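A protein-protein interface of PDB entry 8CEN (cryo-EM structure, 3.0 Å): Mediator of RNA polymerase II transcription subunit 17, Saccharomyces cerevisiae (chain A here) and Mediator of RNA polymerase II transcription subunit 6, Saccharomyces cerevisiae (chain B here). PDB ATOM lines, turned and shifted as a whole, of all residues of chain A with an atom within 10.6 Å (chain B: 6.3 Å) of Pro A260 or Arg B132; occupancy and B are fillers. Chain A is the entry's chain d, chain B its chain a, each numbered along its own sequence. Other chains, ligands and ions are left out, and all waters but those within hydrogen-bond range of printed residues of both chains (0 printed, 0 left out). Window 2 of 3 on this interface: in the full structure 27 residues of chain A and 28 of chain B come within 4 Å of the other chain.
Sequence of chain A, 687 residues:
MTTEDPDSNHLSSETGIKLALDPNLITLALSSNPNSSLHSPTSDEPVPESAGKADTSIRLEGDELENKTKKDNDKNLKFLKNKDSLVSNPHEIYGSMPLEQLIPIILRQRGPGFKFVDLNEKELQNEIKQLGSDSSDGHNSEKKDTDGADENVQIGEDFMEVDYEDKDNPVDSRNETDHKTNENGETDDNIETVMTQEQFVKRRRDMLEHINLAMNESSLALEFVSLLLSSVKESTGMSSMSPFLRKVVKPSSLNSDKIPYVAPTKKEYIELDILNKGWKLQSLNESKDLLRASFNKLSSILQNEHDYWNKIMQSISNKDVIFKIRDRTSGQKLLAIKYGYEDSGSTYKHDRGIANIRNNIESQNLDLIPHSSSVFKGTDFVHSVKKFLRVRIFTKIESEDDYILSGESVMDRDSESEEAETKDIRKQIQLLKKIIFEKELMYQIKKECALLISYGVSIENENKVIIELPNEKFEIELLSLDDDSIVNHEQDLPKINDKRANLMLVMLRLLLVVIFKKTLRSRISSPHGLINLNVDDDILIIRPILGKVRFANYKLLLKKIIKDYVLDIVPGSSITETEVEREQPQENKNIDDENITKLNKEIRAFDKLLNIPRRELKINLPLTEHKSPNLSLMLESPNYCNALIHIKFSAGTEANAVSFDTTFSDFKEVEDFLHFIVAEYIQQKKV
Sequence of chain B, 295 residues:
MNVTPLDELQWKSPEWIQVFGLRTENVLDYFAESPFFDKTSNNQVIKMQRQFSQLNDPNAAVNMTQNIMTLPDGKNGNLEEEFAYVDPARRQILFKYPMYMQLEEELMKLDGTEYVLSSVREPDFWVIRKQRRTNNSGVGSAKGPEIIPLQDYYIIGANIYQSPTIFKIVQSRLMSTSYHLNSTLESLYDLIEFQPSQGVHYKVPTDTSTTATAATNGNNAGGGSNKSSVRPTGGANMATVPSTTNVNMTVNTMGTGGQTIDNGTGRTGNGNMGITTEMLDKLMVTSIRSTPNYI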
ATOM      1  N   ASP A 257     -10.914  28.356 -16.540  1.00  0.00           N
ATOM      2  CA  ASP A 257     -10.447  28.181 -15.172  1.00  0.00           C
ATOM      3  C   ASP A 257      -9.184  28.999 -14.953  1.00  0.00           C
ATOM      4  O   ASP A 257      -8.488  29.377 -15.898  1.00  0.00           O
ATOM      5  CB  ASP A 257     -10.193  26.705 -14.848  1.00  0.00           C
ATOM      6  CG  ASP A 257      -9.141  26.084 -15.742  1.00  0.00           C
ATOM      7  OD1 ASP A 257      -7.948  26.128 -15.380  1.00  0.00           O
ATOM      8  OD2 ASP A 257      -9.508  25.544 -16.804  1.00  0.00           O
ATOM      9  N   LYS A 258      -8.893  29.253 -13.681  1.00  0.00           N
ATOM     10  CA  LYS A 258      -7.784  30.109 -13.277  1.00  0.00           C
ATOM     11  C   LYS A 258      -6.484  29.313 -13.317  1.00  0.00           C
ATOM     12  O   LYS A 258      -6.239  28.468 -12.452  1.00  0.00           O
ATOM     13  CB  LYS A 258      -8.042  30.655 -11.876  1.00  0.00           C
ATOM     14  CG  LYS A 258      -6.981  31.594 -11.318  1.00  0.00           C
ATOM     15  CD  LYS A 258      -6.944  32.938 -12.024  1.00  0.00           C
ATOM     16  CE  LYS A 258      -5.944  33.860 -11.338  1.00  0.00           C
ATOM     17  NZ  LYS A 258      -5.804  35.182 -12.005  1.00  0.00           N
ATOM     18  N   ILE A 259      -5.647  29.579 -14.316  1.00  0.00           N
ATOM     19  CA  ILE A 259      -4.281  29.065 -14.317  1.00  0.00           C
ATOM     20  C   ILE A 259      -3.504  30.034 -13.430  1.00  0.00           C
ATOM     21  O   ILE A 259      -3.958  31.176 -13.257  1.00  0.00           O
ATOM     22  CB  ILE A 259      -3.725  28.937 -15.750  1.00  0.00           C
ATOM     23  CG1 ILE A 259      -3.288  30.287 -16.310  1.00  0.00           C
ATOM     24  CG2 ILE A 259      -4.764  28.311 -16.663  1.00  0.00           C
ATOM     25  CD1 ILE A 259      -2.578  30.187 -17.642  1.00  0.00           C
ATOM     26  N   PRO A 260      -2.383  29.641 -12.814  1.00  0.00           N
ATOM     27  CA  PRO A 260      -1.800  30.472 -11.752  1.00  0.00           C
ATOM     28  C   PRO A 260      -1.253  31.802 -12.246  1.00  0.00           C
ATOM     29  O   PRO A 260      -0.884  31.962 -13.413  1.00  0.00           O
ATOM     30  CB  PRO A 260      -0.674  29.596 -11.191  1.00  0.00           C
ATOM     31  CG  PRO A 260      -0.338  28.668 -12.285  1.00  0.00           C
ATOM     32  CD  PRO A 260      -1.630  28.383 -12.973  1.00  0.00           C
ATOM     33  N   TYR A 261      -1.235  32.766 -11.327  1.00  0.00           N
ATOM     34  CA  TYR A 261      -0.684  34.090 -11.584  1.00  0.00           C
ATOM     35  C   TYR A 261       0.801  33.987 -11.904  1.00  0.00           C
ATOM     36  O   TYR A 261       1.595  33.529 -11.077  1.00  0.00           O
ATOM     37  CB  TYR A 261      -0.916  34.978 -10.359  1.00  0.00           C
ATOM     38  CG  TYR A 261      -0.449  36.413 -10.489  1.00  0.00           C
ATOM     39  CD1 TYR A 261      -1.283  37.390 -11.017  1.00  0.00           C
ATOM     40  CD2 TYR A 261       0.814  36.797 -10.049  1.00  0.00           C
ATOM     41  CE1 TYR A 261      -0.864  38.704 -11.125  1.00  0.00           C
ATOM     42  CE2 TYR A 261       1.241  38.108 -10.156  1.00  0.00           C
ATOM     43  CZ  TYR A 261       0.398  39.056 -10.694  1.00  0.00           C
ATOM     44  OH  TYR A 261       0.820  40.362 -10.799  1.00  0.00           O
ATOM     45  N   VAL A 262       1.173  34.414 -13.107  1.00  0.00           N
ATOM     46  CA  VAL A 262       2.546  34.318 -13.583  1.00  0.00           C
ATOM     47  C   VAL A 262       3.049  35.715 -13.931  1.00  0.00           C
ATOM     48  O   VAL A 262       2.318  36.534 -14.500  1.00  0.00           O
ATOM     49  CB  VAL A 262       2.666  33.340 -14.780  1.00  0.00           C
ATOM     50  CG1 VAL A 262       1.837  33.794 -15.982  1.00  0.00           C
ATOM     51  CG2 VAL A 262       4.124  33.131 -15.172  1.00  0.00           C
ATOM     52  N   ALA A 263       4.274  36.005 -13.516  1.00  0.00           N
ATOM     53  CA  ALA A 263       4.933  37.243 -13.907  1.00  0.00           C
ATOM     54  C   ALA A 263       5.673  37.028 -15.220  1.00  0.00           C
ATOM     55  O   ALA A 263       6.460  36.080 -15.326  1.00  0.00           O
ATOM     56  CB  ALA A 263       5.906  37.708 -12.834  1.00  0.00           C
ATOM     57  N   PRO A 264       5.420  37.852 -16.238  1.00  0.00           N
ATOM     58  CA  PRO A 264       6.120  37.683 -17.517  1.00  0.00           C
ATOM     59  C   PRO A 264       7.615  37.932 -17.372  1.00  0.00           C
ATOM     60  O   PRO A 264       8.058  38.736 -16.551  1.00  0.00           O
ATOM     61  CB  PRO A 264       5.460  38.730 -18.423  1.00  0.00           C
ATOM     62  CG  PRO A 264       4.163  39.065 -17.763  1.00  0.00           C
ATOM     63  CD  PRO A 264       4.399  38.910 -16.296  1.00  0.00           C
ATOM     64  N   GLY B 112       2.922  17.273  -7.417  1.00  0.00           N
ATOM     65  CA  GLY B 112       3.508  18.015  -8.515  1.00  0.00           C
ATOM     66  C   GLY B 112       2.697  18.020  -9.794  1.00  0.00           C
ATOM     67  O   GLY B 112       1.474  17.858  -9.770  1.00  0.00           O
ATOM     68  N   THR B 113       3.383  18.199 -10.920  1.00  0.00           N
ATOM     69  CA  THR B 113       2.718  18.354 -12.207  1.00  0.00           C
ATOM     70  C   THR B 113       2.125  17.035 -12.699  1.00  0.00           C
ATOM     71  O   THR B 113       2.714  15.966 -12.533  1.00  0.00           O
ATOM     72  CB  THR B 113       3.702  18.932 -13.232  1.00  0.00           C
ATOM     73  OG1 THR B 113       3.044  19.122 -14.488  1.00  0.00           O
ATOM     74  CG2 THR B 113       4.941  18.052 -13.408  1.00  0.00           C
ATOM     75  N   GLU B 114       0.934  17.119 -13.289  1.00  0.00           N
ATOM     76  CA  GLU B 114       0.238  15.944 -13.793  1.00  0.00           C
ATOM     77  C   GLU B 114      -0.777  16.391 -14.832  1.00  0.00           C
ATOM     78  O   GLU B 114      -1.084  17.579 -14.954  1.00  0.00           O
ATOM     79  CB  GLU B 114      -0.461  15.168 -12.670  1.00  0.00           C
ATOM     80  CG  GLU B 114      -1.642  15.904 -12.058  1.00  0.00           C
ATOM     81  CD  GLU B 114      -2.079  15.316 -10.732  1.00  0.00           C
ATOM     82  OE1 GLU B 114      -1.420  14.372 -10.251  1.00  0.00           O
ATOM     83  OE2 GLU B 114      -3.084  15.800 -10.170  1.00  0.00           O
ATOM     84  N   LYS B 130      -3.580  20.327 -17.281  1.00  0.00           N
ATOM     85  CA  LYS B 130      -2.391  20.388 -16.445  1.00  0.00           C
ATOM     86  C   LYS B 130      -2.810  20.723 -15.018  1.00  0.00           C
ATOM     87  O   LYS B 130      -3.708  21.540 -14.798  1.00  0.00           O
ATOM     88  CB  LYS B 130      -1.432  21.457 -16.975  1.00  0.00           C
ATOM     89  CG  LYS B 130      -0.162  21.654 -16.161  1.00  0.00           C
ATOM     90  CD  LYS B 130       0.805  20.526 -16.282  1.00  0.00           C
ATOM     91  CE  LYS B 130       1.481  20.593 -17.629  1.00  0.00           C
ATOM     92  NZ  LYS B 130       2.370  21.784 -17.740  1.00  0.00           N
ATOM     93  N   GLN B 131      -2.156  20.100 -14.043  1.00  0.00           N
ATOM     94  CA  GLN B 131      -2.632  20.184 -12.671  1.00  0.00           C
ATOM     95  C   GLN B 131      -1.470  19.967 -11.713  1.00  0.00           C
ATOM     96  O   GLN B 131      -0.698  19.022 -11.888  1.00  0.00           O
ATOM     97  CB  GLN B 131      -3.727  19.137 -12.449  1.00  0.00           C
ATOM     98  CG  GLN B 131      -4.202  18.958 -11.031  1.00  0.00           C
ATOM     99  CD  GLN B 131      -5.590  18.350 -10.984  1.00  0.00           C
ATOM    100  OE1 GLN B 131      -6.585  19.032 -11.221  1.00  0.00           O
ATOM    101  NE2 GLN B 131      -5.660  17.059 -10.685  1.00  0.00           N
ATOM    102  N   ARG B 132      -1.337  20.836 -10.715  1.00  0.00           N
ATOM    103  CA  ARG B 132      -0.381  20.627  -9.636  1.00  0.00           C
ATOM    104  C   ARG B 132      -1.113  20.279  -8.349  1.00  0.00           C
ATOM    105  O   ARG B 132      -2.085  20.941  -7.972  1.00  0.00           O
ATOM    106  CB  ARG B 132       0.525  21.846  -9.418  1.00  0.00           C
ATOM    107  CG  ARG B 132       1.470  22.122 -10.575  1.00  0.00           C
ATOM    108  CD  ARG B 132       2.349  23.345 -10.339  1.00  0.00           C
ATOM    109  NE  ARG B 132       1.620  24.606 -10.316  1.00  0.00           N
ATOM    110  CZ  ARG B 132       2.164  25.771  -9.994  1.00  0.00           C
ATOM    111  NH1 ARG B 132       3.436  25.864  -9.641  1.00  0.00           N
ATOM    112  NH2 ARG B 132       1.419  26.870 -10.030  1.00  0.00           N
ATOM    113  N   ARG B 133      -0.630  19.237  -7.679  1.00  0.00           N
ATOM    114  CA  ARG B 133      -1.263  18.683  -6.492  1.00  0.00           C
ATOM    115  C   ARG B 133      -0.294  18.736  -5.319  1.00  0.00           C
ATOM    116  O   ARG B 133       0.885  18.399  -5.460  1.00  0.00           O
ATOM    117  CB  ARG B 133      -1.705  17.238  -6.743  1.00  0.00           C
ATOM    118  CG  ARG B 133      -2.360  16.553  -5.556  1.00  0.00           C
ATOM    119  CD  ARG B 133      -2.464  15.058  -5.796  1.00  0.00           C
ATOM    120  NE  ARG B 133      -2.905  14.758  -7.152  1.00  0.00           N
ATOM    121  CZ  ARG B 133      -4.096  14.266  -7.463  1.00  0.00           C
ATOM    122  NH1 ARG B 133      -4.998  13.999  -6.534  1.00  0.00           N
ATOM    123  NH2 ARG B 133      -4.388  14.035  -8.739  1.00  0.00           N
ATOM    124  N   THR B 134      -0.795  19.172  -4.165  1.00  0.00           N
ATOM    125  CA  THR B 134      -0.034  19.172  -2.926  1.00  0.00           C
ATOM    126  C   THR B 134      -0.862  18.525  -1.827  1.00  0.00           C
ATOM    127  O   THR B 134      -2.088  18.655  -1.795  1.00  0.00           O
ATOM    128  CB  THR B 134       0.367  20.591  -2.494  1.00  0.00           C
ATOM    129  OG1 THR B 134      -0.796  21.430  -2.462  1.00  0.00           O
ATOM    130  CG2 THR B 134       1.393  21.182  -3.450  1.00  0.00           C
ATOM    131  N   GLU B 146      -4.507  19.630  -1.827  1.00  0.00           N
ATOM    132  CA  GLU B 146      -4.741  20.980  -2.321  1.00  0.00           C
ATOM    133  C   GLU B 146      -4.312  21.037  -3.781  1.00  0.00           C
ATOM    134  O   GLU B 146      -3.141  20.802  -4.098  1.00  0.00           O
ATOM    135  CB  GLU B 146      -3.976  22.002  -1.481  1.00  0.00           C
ATOM    136  CG  GLU B 146      -4.423  23.441  -1.670  1.00  0.00           C
ATOM    137  CD  GLU B 146      -3.590  24.189  -2.688  1.00  0.00           C
ATOM    138  OE1 GLU B 146      -2.384  23.892  -2.811  1.00  0.00           O
ATOM    139  OE2 GLU B 146      -4.144  25.086  -3.356  1.00  0.00           O
ATOM    140  N   ILE B 147      -5.257  21.347  -4.665  1.00  0.00           N
ATOM    141  CA  ILE B 147      -5.057  21.259  -6.105  1.00  0.00           C
ATOM    142  C   ILE B 147      -5.318  22.624  -6.726  1.00  0.00           C
ATOM    143  O   ILE B 147      -6.367  23.233  -6.482  1.00  0.00           O
ATOM    144  CB  ILE B 147      -5.965  20.182  -6.731  1.00  0.00           C
ATOM    145  CG1 ILE B 147      -5.379  18.790  -6.495  1.00  0.00           C
ATOM    146  CG2 ILE B 147      -6.177  20.424  -8.216  1.00  0.00           C
ATOM    147  CD1 ILE B 147      -6.376  17.678  -6.679  1.00  0.00           C
ATOM    148  N   ILE B 148      -4.361  23.103  -7.515  1.00  0.00           N
ATOM    149  CA  ILE B 148      -4.555  24.291  -8.341  1.00  0.00           C
ATOM    150  C   ILE B 148      -4.427  23.883  -9.805  1.00  0.00           C
ATOM    151  O   ILE B 148      -3.603  23.022 -10.143  1.00  0.00           O
ATOM    152  CB  ILE B 148      -3.578  25.415  -7.952  1.00  0.00           C
ATOM    153  CG1 ILE B 148      -2.122  24.993  -8.159  1.00  0.00           C
ATOM    154  CG2 ILE B 148      -3.816  25.858  -6.520  1.00  0.00           C
ATOM    155  CD1 ILE B 148      -1.142  26.125  -8.012  1.00  0.00           C
ATOM    156  N   PRO B 149      -5.251  24.425 -10.694  1.00  0.00           N
ATOM    157  CA  PRO B 149      -5.215  24.010 -12.096  1.00  0.00           C
ATOM    158  C   PRO B 149      -4.257  24.866 -12.915  1.00  0.00           C
ATOM    159  O   PRO B 149      -3.764  25.905 -12.471  1.00  0.00           O
ATOM    160  CB  PRO B 149      -6.662  24.222 -12.554  1.00  0.00           C
ATOM    161  CG  PRO B 149      -7.134  25.359 -11.726  1.00  0.00           C
ATOM    162  CD  PRO B 149      -6.419  25.274 -10.400  1.00  0.00           C
ATOM    163  N   LEU B 150      -4.002  24.399 -14.130  1.00  0.00           N
ATOM    164  CA  LEU B 150      -3.164  25.104 -15.092  1.00  0.00           C
ATOM    165  C   LEU B 150      -3.815  24.928 -16.459  1.00  0.00           C
ATOM    166  O   LEU B 150      -5.011  24.633 -16.556  1.00  0.00           O
ATOM    167  CB  LEU B 150      -1.711  24.614 -15.060  1.00  0.00           C
ATOM    168  CG  LEU B 150      -0.769  24.924 -13.894  1.00  0.00           C
ATOM    169  CD1 LEU B 150      -0.915  23.916 -12.770  1.00  0.00           C
ATOM    170  CD2 LEU B 150       0.671  24.981 -14.378  1.00  0.00           C
ATOM    171  N   GLN B 151      -3.031  25.147 -17.514  1.00  0.00           N
ATOM    172  CA  GLN B 151      -3.542  25.193 -18.879  1.00  0.00           C
ATOM    173  C   GLN B 151      -4.204  23.878 -19.284  1.00  0.00           C
ATOM    174  O   GLN B 151      -3.818  22.791 -18.843  1.00  0.00           O
ATOM    175  CB  GLN B 151      -2.402  25.524 -19.843  1.00  0.00           C
ATOM    176  CG  GLN B 151      -1.842  26.928 -19.668  1.00  0.00           C
ATOM    177  CD  GLN B 151      -0.700  27.221 -20.616  1.00  0.00           C
ATOM    178  OE1 GLN B 151      -0.270  26.354 -21.372  1.00  0.00           O
ATOM    179  NE2 GLN B 151      -0.198  28.450 -20.578  1.00  0.00           N
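The side-chain carboxylate (OD1) of Asp A257 lies close to the backbone carbonyl oxygen (O) of Leu B150, at 3.5 Å.
The backbone carbonyl oxygen (O) of Lys B130 lies within hydrogen-bond range of the backbone NH (N) of Leu B150, 3.0 Å away. The backbone NH of Lys B130 is in hydrogen-bond range of the backbone carbonyl oxygen of Gln B151, 2.9 Å away. The backbone carbonyl oxygen of Arg B132 lies within hydrogen-bond range of the backbone NH of Ile B148 (3.2 Å).
Among the printed residues, merely in contact across the chains: Pro A260 with Pro B149, Lys A258 with Pro B149, Pro A260 with Arg B132, Ile A259 with Leu B150, Asp A257 with Pro B149, Pro A260 with Leu B150, Ile A259 with Pro B149 and Ile A259 with Gln B151.
Arg B132 touches just one residue of chain A: Pro A260 (3.4 Å). Thr B113 touches none of the printed residues of chain A. No residue of chain A comes within 4 Å of Glu B114. No residue of chain A comes within 4 Å of Ile B147. Pro B149 touches just these residues of chain A: Asp A257, Lys A258, Ile A259 and Pro A260. Of chain A, only Asp A257 (3.5 Å), Ile A259 (3.5 Å) and Pro A260 (3.7 Å) come within 4 Å of Leu B150. Of the printed residues of chain B, Lys A258 touches Pro B149 (3.3 Å). Of the printed residues of chain A, Gln B151 touches Ile A259. Printed residues of chain B within 4 Å of Asp A257: Pro B149 and Leu B150. The nearest residue of chain A that does not touch Arg B132 is Tyr A261 (6.6 Å).
Of the 8 printed residues of chain A, 4 touch a printed residue of chain B. Hydrophobic or aromatic side chains of chain A that line the printed part of chain B: Ile A259 and Pro A260. Of the 14 printed residues of chain B, 4 touch a printed residue of chain A. Printed residues of chain B that touch a printed residue of chain A: Arg B132, Pro B149, Leu B150 and Gln B151. Among the printed residues, 9 pairs touch across the chains. Among the printed residues, no Asp or Glu carboxylate lies within 4 Å of a Lys or Arg side-chain nitrogen of the other chain.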
